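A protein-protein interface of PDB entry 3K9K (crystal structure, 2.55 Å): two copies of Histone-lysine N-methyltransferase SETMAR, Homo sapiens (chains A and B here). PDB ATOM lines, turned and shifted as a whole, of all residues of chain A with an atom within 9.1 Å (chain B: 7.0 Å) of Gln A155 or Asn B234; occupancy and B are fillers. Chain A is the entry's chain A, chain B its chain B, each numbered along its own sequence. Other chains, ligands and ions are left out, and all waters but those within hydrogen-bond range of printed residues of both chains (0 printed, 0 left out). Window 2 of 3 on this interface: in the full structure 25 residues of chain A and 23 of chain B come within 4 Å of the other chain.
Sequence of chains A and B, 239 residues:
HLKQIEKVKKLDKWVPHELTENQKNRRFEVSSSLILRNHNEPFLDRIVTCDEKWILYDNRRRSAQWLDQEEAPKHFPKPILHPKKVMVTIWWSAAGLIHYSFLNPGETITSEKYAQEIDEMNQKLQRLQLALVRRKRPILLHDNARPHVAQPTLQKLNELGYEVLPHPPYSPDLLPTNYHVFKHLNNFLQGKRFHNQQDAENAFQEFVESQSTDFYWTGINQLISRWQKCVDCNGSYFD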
ATOM      1  N   SER A 111     -22.476  -5.472  29.274  1.00  0.00           N
ATOM      2  CA  SER A 111     -22.323  -6.283  28.070  1.00  0.00           C
ATOM      3  C   SER A 111     -23.679  -6.764  27.561  1.00  0.00           C
ATOM      4  O   SER A 111     -23.913  -6.823  26.352  1.00  0.00           O
ATOM      5  CB  SER A 111     -21.403  -7.474  28.329  1.00  0.00           C
ATOM      6  OG  SER A 111     -21.193  -8.200  27.138  1.00  0.00           O
ATOM      7  N   ALA A 115     -25.440  -5.686  24.248  1.00  0.00           N
ATOM      8  CA  ALA A 115     -25.997  -6.721  23.398  1.00  0.00           C
ATOM      9  C   ALA A 115     -27.387  -6.332  22.922  1.00  0.00           C
ATOM     10  O   ALA A 115     -27.718  -6.477  21.742  1.00  0.00           O
ATOM     11  CB  ALA A 115     -26.048  -8.023  24.137  1.00  0.00           C
ATOM     12  N   ILE A 118     -27.125  -3.617  20.359  1.00  0.00           N
ATOM     13  CA  ILE A 118     -26.828  -4.224  19.066  1.00  0.00           C
ATOM     14  C   ILE A 118     -28.083  -4.754  18.372  1.00  0.00           C
ATOM     15  O   ILE A 118     -28.307  -4.514  17.184  1.00  0.00           O
ATOM     16  CB  ILE A 118     -25.843  -5.400  19.221  1.00  0.00           C
ATOM     17  CG1 ILE A 118     -24.466  -4.893  19.637  1.00  0.00           C
ATOM     18  CG2 ILE A 118     -25.758  -6.190  17.925  1.00  0.00           C
ATOM     19  CD1 ILE A 118     -23.532  -5.992  20.079  1.00  0.00           C
ATOM     20  N   ASP A 119     -28.892  -5.492  19.128  1.00  0.00           N
ATOM     21  CA  ASP A 119     -30.111  -6.090  18.609  1.00  0.00           C
ATOM     22  C   ASP A 119     -31.053  -5.009  18.099  1.00  0.00           C
ATOM     23  O   ASP A 119     -31.704  -5.182  17.067  1.00  0.00           O
ATOM     24  CB  ASP A 119     -30.786  -6.920  19.698  1.00  0.00           C
ATOM     25  CG  ASP A 119     -31.242  -8.278  19.196  1.00  0.00           C
ATOM     26  OD1 ASP A 119     -31.739  -8.354  18.044  1.00  0.00           O
ATOM     27  OD2 ASP A 119     -31.097  -9.269  19.953  1.00  0.00           O
ATOM     28  N   HIS A 148     -17.523  -3.860  28.343  1.00  0.00           N
ATOM     29  CA  HIS A 148     -18.862  -4.357  28.063  1.00  0.00           C
ATOM     30  C   HIS A 148     -18.897  -5.144  26.754  1.00  0.00           C
ATOM     31  O   HIS A 148     -19.960  -5.590  26.305  1.00  0.00           O
ATOM     32  CB  HIS A 148     -19.842  -3.200  27.997  1.00  0.00           C
ATOM     33  CG  HIS A 148     -19.405  -2.104  27.083  1.00  0.00           C
ATOM     34  ND1 HIS A 148     -19.939  -1.930  25.823  1.00  0.00           N
ATOM     35  CD2 HIS A 148     -18.482  -1.130  27.239  1.00  0.00           C
ATOM     36  CE1 HIS A 148     -19.367  -0.889  25.248  1.00  0.00           C
ATOM     37  NE2 HIS A 148     -18.480  -0.383  26.085  1.00  0.00           N
ATOM     38  N   VAL A 149     -17.729  -5.285  26.132  1.00  0.00           N
ATOM     39  CA  VAL A 149     -17.559  -6.221  25.032  1.00  0.00           C
ATOM     40  C   VAL A 149     -17.098  -7.544  25.634  1.00  0.00           C
ATOM     41  O   VAL A 149     -15.901  -7.784  25.799  1.00  0.00           O
ATOM     42  CB  VAL A 149     -16.531  -5.724  24.001  1.00  0.00           C
ATOM     43  CG1 VAL A 149     -16.270  -6.797  22.990  1.00  0.00           C
ATOM     44  CG2 VAL A 149     -17.027  -4.468  23.309  1.00  0.00           C
ATOM     45  N   ALA A 150     -18.061  -8.385  25.997  1.00  0.00           N
ATOM     46  CA  ALA A 150     -17.767  -9.671  26.608  1.00  0.00           C
ATOM     47  C   ALA A 150     -18.743 -10.718  26.101  1.00  0.00           C
ATOM     48  O   ALA A 150     -19.548 -10.452  25.209  1.00  0.00           O
ATOM     49  CB  ALA A 150     -17.819  -9.578  28.126  1.00  0.00           C
ATOM     50  N   GLN A 151     -18.675 -11.906  26.685  1.00  0.00           N
ATOM     51  CA  GLN A 151     -19.404 -13.054  26.166  1.00  0.00           C
ATOM     52  C   GLN A 151     -20.791 -12.730  25.592  1.00  0.00           C
ATOM     53  O   GLN A 151     -21.064 -13.079  24.443  1.00  0.00           O
ATOM     54  CB  GLN A 151     -19.476 -14.165  27.215  1.00  0.00           C
ATOM     55  CG  GLN A 151     -19.475 -15.561  26.609  1.00  0.00           C
ATOM     56  CD  GLN A 151     -18.605 -15.667  25.356  1.00  0.00           C
ATOM     57  OE1 GLN A 151     -17.376 -15.797  25.431  1.00  0.00           O
ATOM     58  NE2 GLN A 151     -19.250 -15.620  24.194  1.00  0.00           N
ATOM     59  N   PRO A 152     -21.662 -12.055  26.377  1.00  0.00           N
ATOM     60  CA  PRO A 152     -23.032 -11.728  25.919  1.00  0.00           C
ATOM     61  C   PRO A 152     -23.067 -10.910  24.629  1.00  0.00           C
ATOM     62  O   PRO A 152     -23.817 -11.235  23.701  1.00  0.00           O
ATOM     63  CB  PRO A 152     -23.605 -10.902  27.072  1.00  0.00           C
ATOM     64  CG  PRO A 152     -22.799 -11.323  28.276  1.00  0.00           C
ATOM     65  CD  PRO A 152     -21.416 -11.603  27.760  1.00  0.00           C
ATOM     66  N   THR A 153     -22.268  -9.851  24.578  1.00  0.00           N
ATOM     67  CA  THR A 153     -22.097  -9.080  23.353  1.00  0.00           C
ATOM     68  C   THR A 153     -21.573  -9.958  22.216  1.00  0.00           C
ATOM     69  O   THR A 153     -22.122  -9.957  21.116  1.00  0.00           O
ATOM     70  CB  THR A 153     -21.096  -7.937  23.547  1.00  0.00           C
ATOM     71  OG1 THR A 153     -21.539  -7.089  24.613  1.00  0.00           O
ATOM     72  CG2 THR A 153     -20.960  -7.129  22.258  1.00  0.00           C
ATOM     73  N   LEU A 154     -20.504 -10.707  22.480  1.00  0.00           N
ATOM     74  CA  LEU A 154     -19.937 -11.574  21.451  1.00  0.00           C
ATOM     75  C   LEU A 154     -20.987 -12.549  20.938  1.00  0.00           C
ATOM     76  O   LEU A 154     -21.157 -12.710  19.732  1.00  0.00           O
ATOM     77  CB  LEU A 154     -18.714 -12.318  21.973  1.00  0.00           C
ATOM     78  CG  LEU A 154     -17.598 -11.407  22.482  1.00  0.00           C
ATOM     79  CD1 LEU A 154     -16.394 -12.209  22.934  1.00  0.00           C
ATOM     80  CD2 LEU A 154     -17.215 -10.431  21.415  1.00  0.00           C
ATOM     81  N   GLN A 155     -21.706 -13.176  21.864  1.00  0.00           N
ATOM     82  CA  GLN A 155     -22.762 -14.116  21.522  1.00  0.00           C
ATOM     83  C   GLN A 155     -23.773 -13.486  20.566  1.00  0.00           C
ATOM     84  O   GLN A 155     -24.200 -14.100  19.593  1.00  0.00           O
ATOM     85  CB  GLN A 155     -23.479 -14.557  22.788  1.00  0.00           C
ATOM     86  CG  GLN A 155     -23.677 -16.046  22.904  1.00  0.00           C
ATOM     87  CD  GLN A 155     -22.522 -16.723  23.610  1.00  0.00           C
ATOM     88  OE1 GLN A 155     -22.151 -16.345  24.727  1.00  0.00           O
ATOM     89  NE2 GLN A 155     -21.949 -17.736  22.970  1.00  0.00           N
ATOM     90  N   LYS A 156     -24.153 -12.248  20.841  1.00  0.00           N
ATOM     91  CA  LYS A 156     -25.164 -11.585  20.028  1.00  0.00           C
ATOM     92  C   LYS A 156     -24.687 -11.313  18.606  1.00  0.00           C
ATOM     93  O   LYS A 156     -25.436 -11.497  17.645  1.00  0.00           O
ATOM     94  CB  LYS A 156     -25.615 -10.279  20.690  1.00  0.00           C
ATOM     95  CG  LYS A 156     -26.523  -9.423  19.816  1.00  0.00           C
ATOM     96  CD  LYS A 156     -27.899 -10.040  19.676  1.00  0.00           C
ATOM     97  CE  LYS A 156     -28.503 -10.290  21.049  1.00  0.00           C
ATOM     98  NZ  LYS A 156     -29.726 -11.131  20.977  1.00  0.00           N
ATOM     99  N   LEU A 157     -23.447 -10.852  18.476  1.00  0.00           N
ATOM    100  CA  LEU A 157     -22.876 -10.561  17.166  1.00  0.00           C
ATOM    101  C   LEU A 157     -22.786 -11.843  16.368  1.00  0.00           C
ATOM    102  O   LEU A 157     -23.050 -11.873  15.162  1.00  0.00           O
ATOM    103  CB  LEU A 157     -21.476  -9.981  17.324  1.00  0.00           C
ATOM    104  CG  LEU A 157     -21.398  -8.545  17.821  1.00  0.00           C
ATOM    105  CD1 LEU A 157     -19.987  -8.236  18.269  1.00  0.00           C
ATOM    106  CD2 LEU A 157     -21.858  -7.618  16.717  1.00  0.00           C
ATOM    107  N   ASN A 158     -22.388 -12.906  17.054  1.00  0.00           N
ATOM    108  CA  ASN A 158     -22.286 -14.189  16.418  1.00  0.00           C
ATOM    109  C   ASN A 158     -23.660 -14.635  15.982  1.00  0.00           C
ATOM    110  O   ASN A 158     -23.904 -14.879  14.799  1.00  0.00           O
ATOM    111  CB  ASN A 158     -21.707 -15.220  17.374  1.00  0.00           C
ATOM    112  CG  ASN A 158     -21.599 -16.575  16.731  1.00  0.00           C
ATOM    113  OD1 ASN A 158     -21.049 -16.701  15.638  1.00  0.00           O
ATOM    114  ND2 ASN A 158     -22.151 -17.593  17.382  1.00  0.00           N
ATOM    115  N   GLU A 159     -24.555 -14.731  16.961  1.00  0.00           N
ATOM    116  CA  GLU A 159     -25.939 -15.110  16.724  1.00  0.00           C
ATOM    117  C   GLU A 159     -26.600 -14.337  15.564  1.00  0.00           C
ATOM    118  O   GLU A 159     -27.515 -14.837  14.923  1.00  0.00           O
ATOM    119  CB  GLU A 159     -26.729 -14.955  18.024  1.00  0.00           C
ATOM    120  CG  GLU A 159     -28.234 -15.013  17.863  1.00  0.00           C
ATOM    121  CD  GLU A 159     -28.970 -14.119  18.863  1.00  0.00           C
ATOM    122  OE1 GLU A 159     -28.427 -13.855  19.971  1.00  0.00           O
ATOM    123  OE2 GLU A 159     -30.097 -13.677  18.536  1.00  0.00           O
ATOM    124  N   LEU A 160     -26.125 -13.129  15.282  1.00  0.00           N
ATOM    125  CA  LEU A 160     -26.714 -12.301  14.231  1.00  0.00           C
ATOM    126  C   LEU A 160     -25.948 -12.341  12.914  1.00  0.00           C
ATOM    127  O   LEU A 160     -26.352 -11.710  11.936  1.00  0.00           O
ATOM    128  CB  LEU A 160     -26.829 -10.845  14.696  1.00  0.00           C
ATOM    129  CG  LEU A 160     -27.856 -10.512  15.782  1.00  0.00           C
ATOM    130  CD1 LEU A 160     -27.687  -9.079  16.232  1.00  0.00           C
ATOM    131  CD2 LEU A 160     -29.261 -10.752  15.271  1.00  0.00           C
ATOM    132  N   GLY A 161     -24.839 -13.075  12.880  1.00  0.00           N
ATOM    133  CA  GLY A 161     -24.063 -13.197  11.656  1.00  0.00           C
ATOM    134  C   GLY A 161     -23.230 -11.959  11.373  1.00  0.00           C
ATOM    135  O   GLY A 161     -23.059 -11.547  10.226  1.00  0.00           O
ATOM    136  N   TYR A 162     -22.717 -11.355  12.439  1.00  0.00           N
ATOM    137  CA  TYR A 162     -21.887 -10.171  12.313  1.00  0.00           C
ATOM    138  C   TYR A 162     -20.413 -10.516  12.334  1.00  0.00           C
ATOM    139  O   TYR A 162     -19.900 -11.094  13.294  1.00  0.00           O
ATOM    140  CB  TYR A 162     -22.186  -9.180  13.427  1.00  0.00           C
ATOM    141  CG  TYR A 162     -23.219  -8.152  13.053  1.00  0.00           C
ATOM    142  CD1 TYR A 162     -24.577  -8.426  13.174  1.00  0.00           C
ATOM    143  CD2 TYR A 162     -22.841  -6.900  12.585  1.00  0.00           C
ATOM    144  CE1 TYR A 162     -25.525  -7.484  12.840  1.00  0.00           C
ATOM    145  CE2 TYR A 162     -23.786  -5.951  12.246  1.00  0.00           C
ATOM    146  CZ  TYR A 162     -25.129  -6.248  12.379  1.00  0.00           C
ATOM    147  OH  TYR A 162     -26.081  -5.314  12.045  1.00  0.00           O
ATOM    148  N   GLU B  21     -10.684 -14.964  30.819  1.00  0.00           N
ATOM    149  CA  GLU B  21     -11.970 -14.698  30.200  1.00  0.00           C
ATOM    150  C   GLU B  21     -11.756 -13.871  28.945  1.00  0.00           C
ATOM    151  O   GLU B  21     -12.494 -13.990  27.965  1.00  0.00           O
ATOM    152  CB  GLU B  21     -12.872 -13.934  31.167  1.00  0.00           C
ATOM    153  CG  GLU B  21     -14.318 -14.408  31.166  1.00  0.00           C
ATOM    154  CD  GLU B  21     -14.464 -15.820  31.722  1.00  0.00           C
ATOM    155  OE1 GLU B  21     -13.429 -16.460  32.016  1.00  0.00           O
ATOM    156  OE2 GLU B  21     -15.613 -16.292  31.867  1.00  0.00           O
ATOM    157  N   GLN B  23      -9.157 -13.980  27.107  1.00  0.00           N
ATOM    158  CA  GLN B  23      -8.447 -14.763  26.112  1.00  0.00           C
ATOM    159  C   GLN B  23      -9.421 -15.642  25.350  1.00  0.00           C
ATOM    160  O   GLN B  23      -9.234 -15.896  24.157  1.00  0.00           O
ATOM    161  CB  GLN B  23      -7.353 -15.603  26.769  1.00  0.00           C
ATOM    162  CG  GLN B  23      -6.211 -14.766  27.301  1.00  0.00           C
ATOM    163  CD  GLN B  23      -5.222 -15.574  28.094  1.00  0.00           C
ATOM    164  OE1 GLN B  23      -5.592 -16.510  28.801  1.00  0.00           O
ATOM    165  NE2 GLN B  23      -3.949 -15.219  27.980  1.00  0.00           N
ATOM    166  N   LYS B  24     -10.463 -16.097  26.041  1.00  0.00           N
ATOM    167  CA  LYS B  24     -11.530 -16.846  25.389  1.00  0.00           C
ATOM    168  C   LYS B  24     -12.388 -15.942  24.505  1.00  0.00           C
ATOM    169  O   LYS B  24     -12.980 -16.397  23.538  1.00  0.00           O
ATOM    170  CB  LYS B  24     -12.398 -17.569  26.415  1.00  0.00           C
ATOM    171  CG  LYS B  24     -11.621 -18.115  27.596  1.00  0.00           C
ATOM    172  CD  LYS B  24     -12.172 -19.453  28.029  1.00  0.00           C
ATOM    173  CE  LYS B  24     -12.106 -19.607  29.529  1.00  0.00           C
ATOM    174  NZ  LYS B  24     -13.172 -18.789  30.175  1.00  0.00           N
ATOM    175  N   ASN B  25     -12.457 -14.661  24.835  1.00  0.00           N
ATOM    176  CA  ASN B  25     -13.244 -13.740  24.034  1.00  0.00           C
ATOM    177  C   ASN B  25     -12.555 -13.511  22.694  1.00  0.00           C
ATOM    178  O   ASN B  25     -13.209 -13.475  21.645  1.00  0.00           O
ATOM    179  CB  ASN B  25     -13.456 -12.412  24.768  1.00  0.00           C
ATOM    180  CG  ASN B  25     -14.238 -12.573  26.069  1.00  0.00           C
ATOM    181  OD1 ASN B  25     -14.048 -11.810  27.022  1.00  0.00           O
ATOM    182  ND2 ASN B  25     -15.121 -13.569  26.112  1.00  0.00           N
ATOM    183  N   ARG B  27     -10.598 -15.527  21.190  1.00  0.00           N
ATOM    184  CA  ARG B  27     -10.697 -16.767  20.424  1.00  0.00           C
ATOM    185  C   ARG B  27     -12.081 -16.908  19.802  1.00  0.00           C
ATOM    186  O   ARG B  27     -12.208 -17.210  18.615  1.00  0.00           O
ATOM    187  CB  ARG B  27     -10.381 -17.978  21.301  1.00  0.00           C
ATOM    188  CG  ARG B  27      -8.935 -18.040  21.768  1.00  0.00           C
ATOM    189  CD  ARG B  27      -8.723 -19.117  22.811  1.00  0.00           C
ATOM    190  NE  ARG B  27      -9.440 -20.348  22.492  1.00  0.00           N
ATOM    191  CZ  ARG B  27      -8.935 -21.349  21.774  1.00  0.00           C
ATOM    192  NH1 ARG B  27      -7.696 -21.266  21.296  1.00  0.00           N
ATOM    193  NH2 ARG B  27      -9.669 -22.429  21.534  1.00  0.00           N
ATOM    194  N   PHE B  28     -13.114 -16.681  20.607  1.00  0.00           N
ATOM    195  CA  PHE B  28     -14.494 -16.752  20.142  1.00  0.00           C
ATOM    196  C   PHE B  28     -14.746 -15.732  19.040  1.00  0.00           C
ATOM    197  O   PHE B  28     -15.329 -16.048  18.000  1.00  0.00           O
ATOM    198  CB  PHE B  28     -15.448 -16.500  21.309  1.00  0.00           C
ATOM    199  CG  PHE B  28     -16.896 -16.679  20.960  1.00  0.00           C
ATOM    200  CD1 PHE B  28     -17.543 -17.867  21.239  1.00  0.00           C
ATOM    201  CD2 PHE B  28     -17.612 -15.653  20.365  1.00  0.00           C
ATOM    202  CE1 PHE B  28     -18.872 -18.040  20.903  1.00  0.00           C
ATOM    203  CE2 PHE B  28     -18.936 -15.811  20.037  1.00  0.00           C
ATOM    204  CZ  PHE B  28     -19.569 -17.014  20.304  1.00  0.00           C
ATOM    205  N   GLN B 228     -15.590 -23.547  14.466  1.00  0.00           N
ATOM    206  CA  GLN B 228     -16.892 -23.850  15.038  1.00  0.00           C
ATOM    207  C   GLN B 228     -16.796 -24.464  16.439  1.00  0.00           C
ATOM    208  O   GLN B 228     -17.527 -24.086  17.355  1.00  0.00           O
ATOM    209  CB  GLN B 228     -17.681 -24.766  14.111  1.00  0.00           C
ATOM    210  CG  GLN B 228     -19.125 -24.908  14.533  1.00  0.00           C
ATOM    211  CD  GLN B 228     -19.863 -23.575  14.552  1.00  0.00           C
ATOM    212  OE1 GLN B 228     -20.016 -22.923  13.519  1.00  0.00           O
ATOM    213  NE2 GLN B 228     -20.331 -23.173  15.731  1.00  0.00           N
ATOM    214  N   LYS B 229     -15.882 -25.407  16.596  1.00  0.00           N
ATOM    215  CA  LYS B 229     -15.722 -26.120  17.851  1.00  0.00           C
ATOM    216  C   LYS B 229     -15.310 -25.146  18.946  1.00  0.00           C
ATOM    217  O   LYS B 229     -15.650 -25.307  20.111  1.00  0.00           O
ATOM    218  CB  LYS B 229     -14.663 -27.213  17.680  1.00  0.00           C
ATOM    219  CG  LYS B 229     -15.058 -28.561  18.249  1.00  0.00           C
ATOM    220  CD  LYS B 229     -14.090 -29.668  17.805  1.00  0.00           C
ATOM    221  CE  LYS B 229     -14.380 -30.188  16.386  1.00  0.00           C
ATOM    222  NZ  LYS B 229     -13.219 -30.982  15.861  1.00  0.00           N
ATOM    223  N   CYS B 230     -14.563 -24.130  18.553  1.00  0.00           N
ATOM    224  CA  CYS B 230     -14.103 -23.103  19.464  1.00  0.00           C
ATOM    225  C   CYS B 230     -15.273 -22.244  19.936  1.00  0.00           C
ATOM    226  O   CYS B 230     -15.453 -22.021  21.129  1.00  0.00           O
ATOM    227  CB  CYS B 230     -13.092 -22.222  18.736  1.00  0.00           C
ATOM    228  SG  CYS B 230     -12.489 -20.841  19.701  1.00  0.00           S
ATOM    229  N   VAL B 231     -16.043 -21.749  18.971  1.00  0.00           N
ATOM    230  CA  VAL B 231     -17.245 -20.977  19.224  1.00  0.00           C
ATOM    231  C   VAL B 231     -18.162 -21.698  20.210  1.00  0.00           C
ATOM    232  O   VAL B 231     -18.568 -21.125  21.218  1.00  0.00           O
ATOM    233  CB  VAL B 231     -18.026 -20.752  17.912  1.00  0.00           C
ATOM    234  CG1 VAL B 231     -19.452 -20.380  18.208  1.00  0.00           C
ATOM    235  CG2 VAL B 231     -17.355 -19.692  17.051  1.00  0.00           C
ATOM    236  N   ASP B 232     -18.481 -22.957  19.916  1.00  0.00           N
ATOM    237  CA  ASP B 232     -19.336 -23.765  20.785  1.00  0.00           C
ATOM    238  C   ASP B 232     -18.808 -23.883  22.210  1.00  0.00           C
ATOM    239  O   ASP B 232     -19.589 -24.008  23.153  1.00  0.00           O
ATOM    240  CB  ASP B 232     -19.519 -25.160  20.203  1.00  0.00           C
ATOM    241  CG  ASP B 232     -20.156 -25.132  18.839  1.00  0.00           C
ATOM    242  OD1 ASP B 232     -20.694 -24.066  18.468  1.00  0.00           O
ATOM    243  OD2 ASP B 232     -20.122 -26.173  18.137  1.00  0.00           O
ATOM    244  N   CYS B 233     -17.488 -23.863  22.363  1.00  0.00           N
ATOM    245  CA  CYS B 233     -16.866 -23.899  23.685  1.00  0.00           C
ATOM    246  C   CYS B 233     -16.744 -22.505  24.262  1.00  0.00           C
ATOM    247  O   CYS B 233     -16.033 -22.294  25.243  1.00  0.00           O
ATOM    248  CB  CYS B 233     -15.480 -24.518  23.595  1.00  0.00           C
ATOM    249  SG  CYS B 233     -15.543 -26.260  23.304  1.00  0.00           S
ATOM    250  N   ASN B 234     -17.437 -21.562  23.631  1.00  0.00           N
ATOM    251  CA  ASN B 234     -17.336 -20.141  23.966  1.00  0.00           C
ATOM    252  C   ASN B 234     -15.898 -19.644  24.053  1.00  0.00           C
ATOM    253  O   ASN B 234     -15.601 -18.698  24.786  1.00  0.00           O
ATOM    254  CB  ASN B 234     -18.109 -19.817  25.251  1.00  0.00           C
ATOM    255  CG  ASN B 234     -19.594 -20.093  25.118  1.00  0.00           C
ATOM    256  OD1 ASN B 234     -20.266 -19.550  24.233  1.00  0.00           O
ATOM    257  ND2 ASN B 234     -20.112 -20.950  25.988  1.00  0.00           N
ATOM    258  N   GLY B 235     -15.009 -20.284  23.301  1.00  0.00           N
ATOM    259  CA  GLY B 235     -13.647 -19.807  23.195  1.00  0.00           C
ATOM    260  C   GLY B 235     -12.655 -20.531  24.081  1.00  0.00           C
ATOM    261  O   GLY B 235     -11.492 -20.148  24.150  1.00  0.00           O
ATOM    262  N   SER B 236     -13.100 -21.579  24.760  1.00  0.00           N
ATOM    263  CA  SER B 236     -12.177 -22.425  25.511  1.00  0.00           C
ATOM    264  C   SER B 236     -11.493 -23.443  24.587  1.00  0.00           C
ATOM    265  O   SER B 236     -11.840 -23.561  23.415  1.00  0.00           O
ATOM    266  CB  SER B 236     -12.919 -23.162  26.633  1.00  0.00           C
ATOM    267  OG  SER B 236     -13.569 -22.257  27.511  1.00  0.00           O
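Printed residues of chain A that touch a printed residue of chain B: Gln A151, Leu A154, Gln A155 and Asn A158. Hydrophobic or aromatic side chains of chain A that line the printed part of chain B: Leu A154. Hydrophobic or aromatic side chains of chain B that line the printed part of chain A: Phe B28 and Val B231. Among the printed residues, no Asp or Glu carboxylate lies within 4 Å of a Lys or Arg side-chain nitrogen of the other chain.
No position is printed for both chains. Of the 8 pairs that touch across the chains among the printed residues, none has its exchanged pair printed and touching as well.
The side-chain amide nitrogen (ND2) of Asn B25 sits at hydrogen-bond distance from the side-chain amide oxygen (OE1) of Gln A151 (3.2 Å). OE1 of Gln A151 sits close to O of Asn B234 (3.5 Å). NE2 of Gln A155 is in hydrogen-bond range of OD1 of Asn B234 (2.8 Å).
Among the printed residues, merely in contact across the chains: Leu A154 with Asn B25 (3.5 Å), Gln A155 with Phe B28 (3.6 Å), Leu A154 with Phe B28 (3.8 Å), Asn A158 with Phe B28 (3.9 Å) and Asn A158 with Val B231 (3.97 Å).
NE2 of Gln A151 lies within hydrogen-bond range of OE1 of Gln A155. The side-chain amide oxygen of Asn B25 lies close to the backbone carbonyl oxygen of Glu B21 (2.8 Å).
Gln A155 touches just these residues of chain B: Phe B28 (3.6 Å) and Asn B234 (2.8 Å). Asn B234 touches just these residues of chain A: Gln A151 and Gln A155. No residue of chain A comes within 4 Å of Gly B235. Of the printed residues of chain B, Leu A154 touches Asn B25 (3.5 Å) and Phe B28 (3.8 Å). Printed residues of chain B within 4 Å of Asn A158: Phe B28 and Val B231. Of the printed residues of chain B, Gln A151 touches Asn B25 (3.2 Å) and Asn B234 (3.5 Å). Printed residues of chain A within 4 Å of Val B231: Asn A158 (3.97 Å). Of the printed residues of chain A, Phe B28 touches Leu A154 (3.8 Å), Gln A155 (3.6 Å) and Asn A158 (3.9 Å). Gln B23 touches none of the printed residues of chain A. Ala A115 touches none of the printed residues of chain B. The nearest residue of chain B that does not touch Gln A155 is Val B231 (5.1 Å). The nearest residue of chain A that does not touch Asn B234 is Leu A154 (6.8 Å). The nearest printed residue of chain B that does not touch Leu A154 is Lys B24 (5.4 Å).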
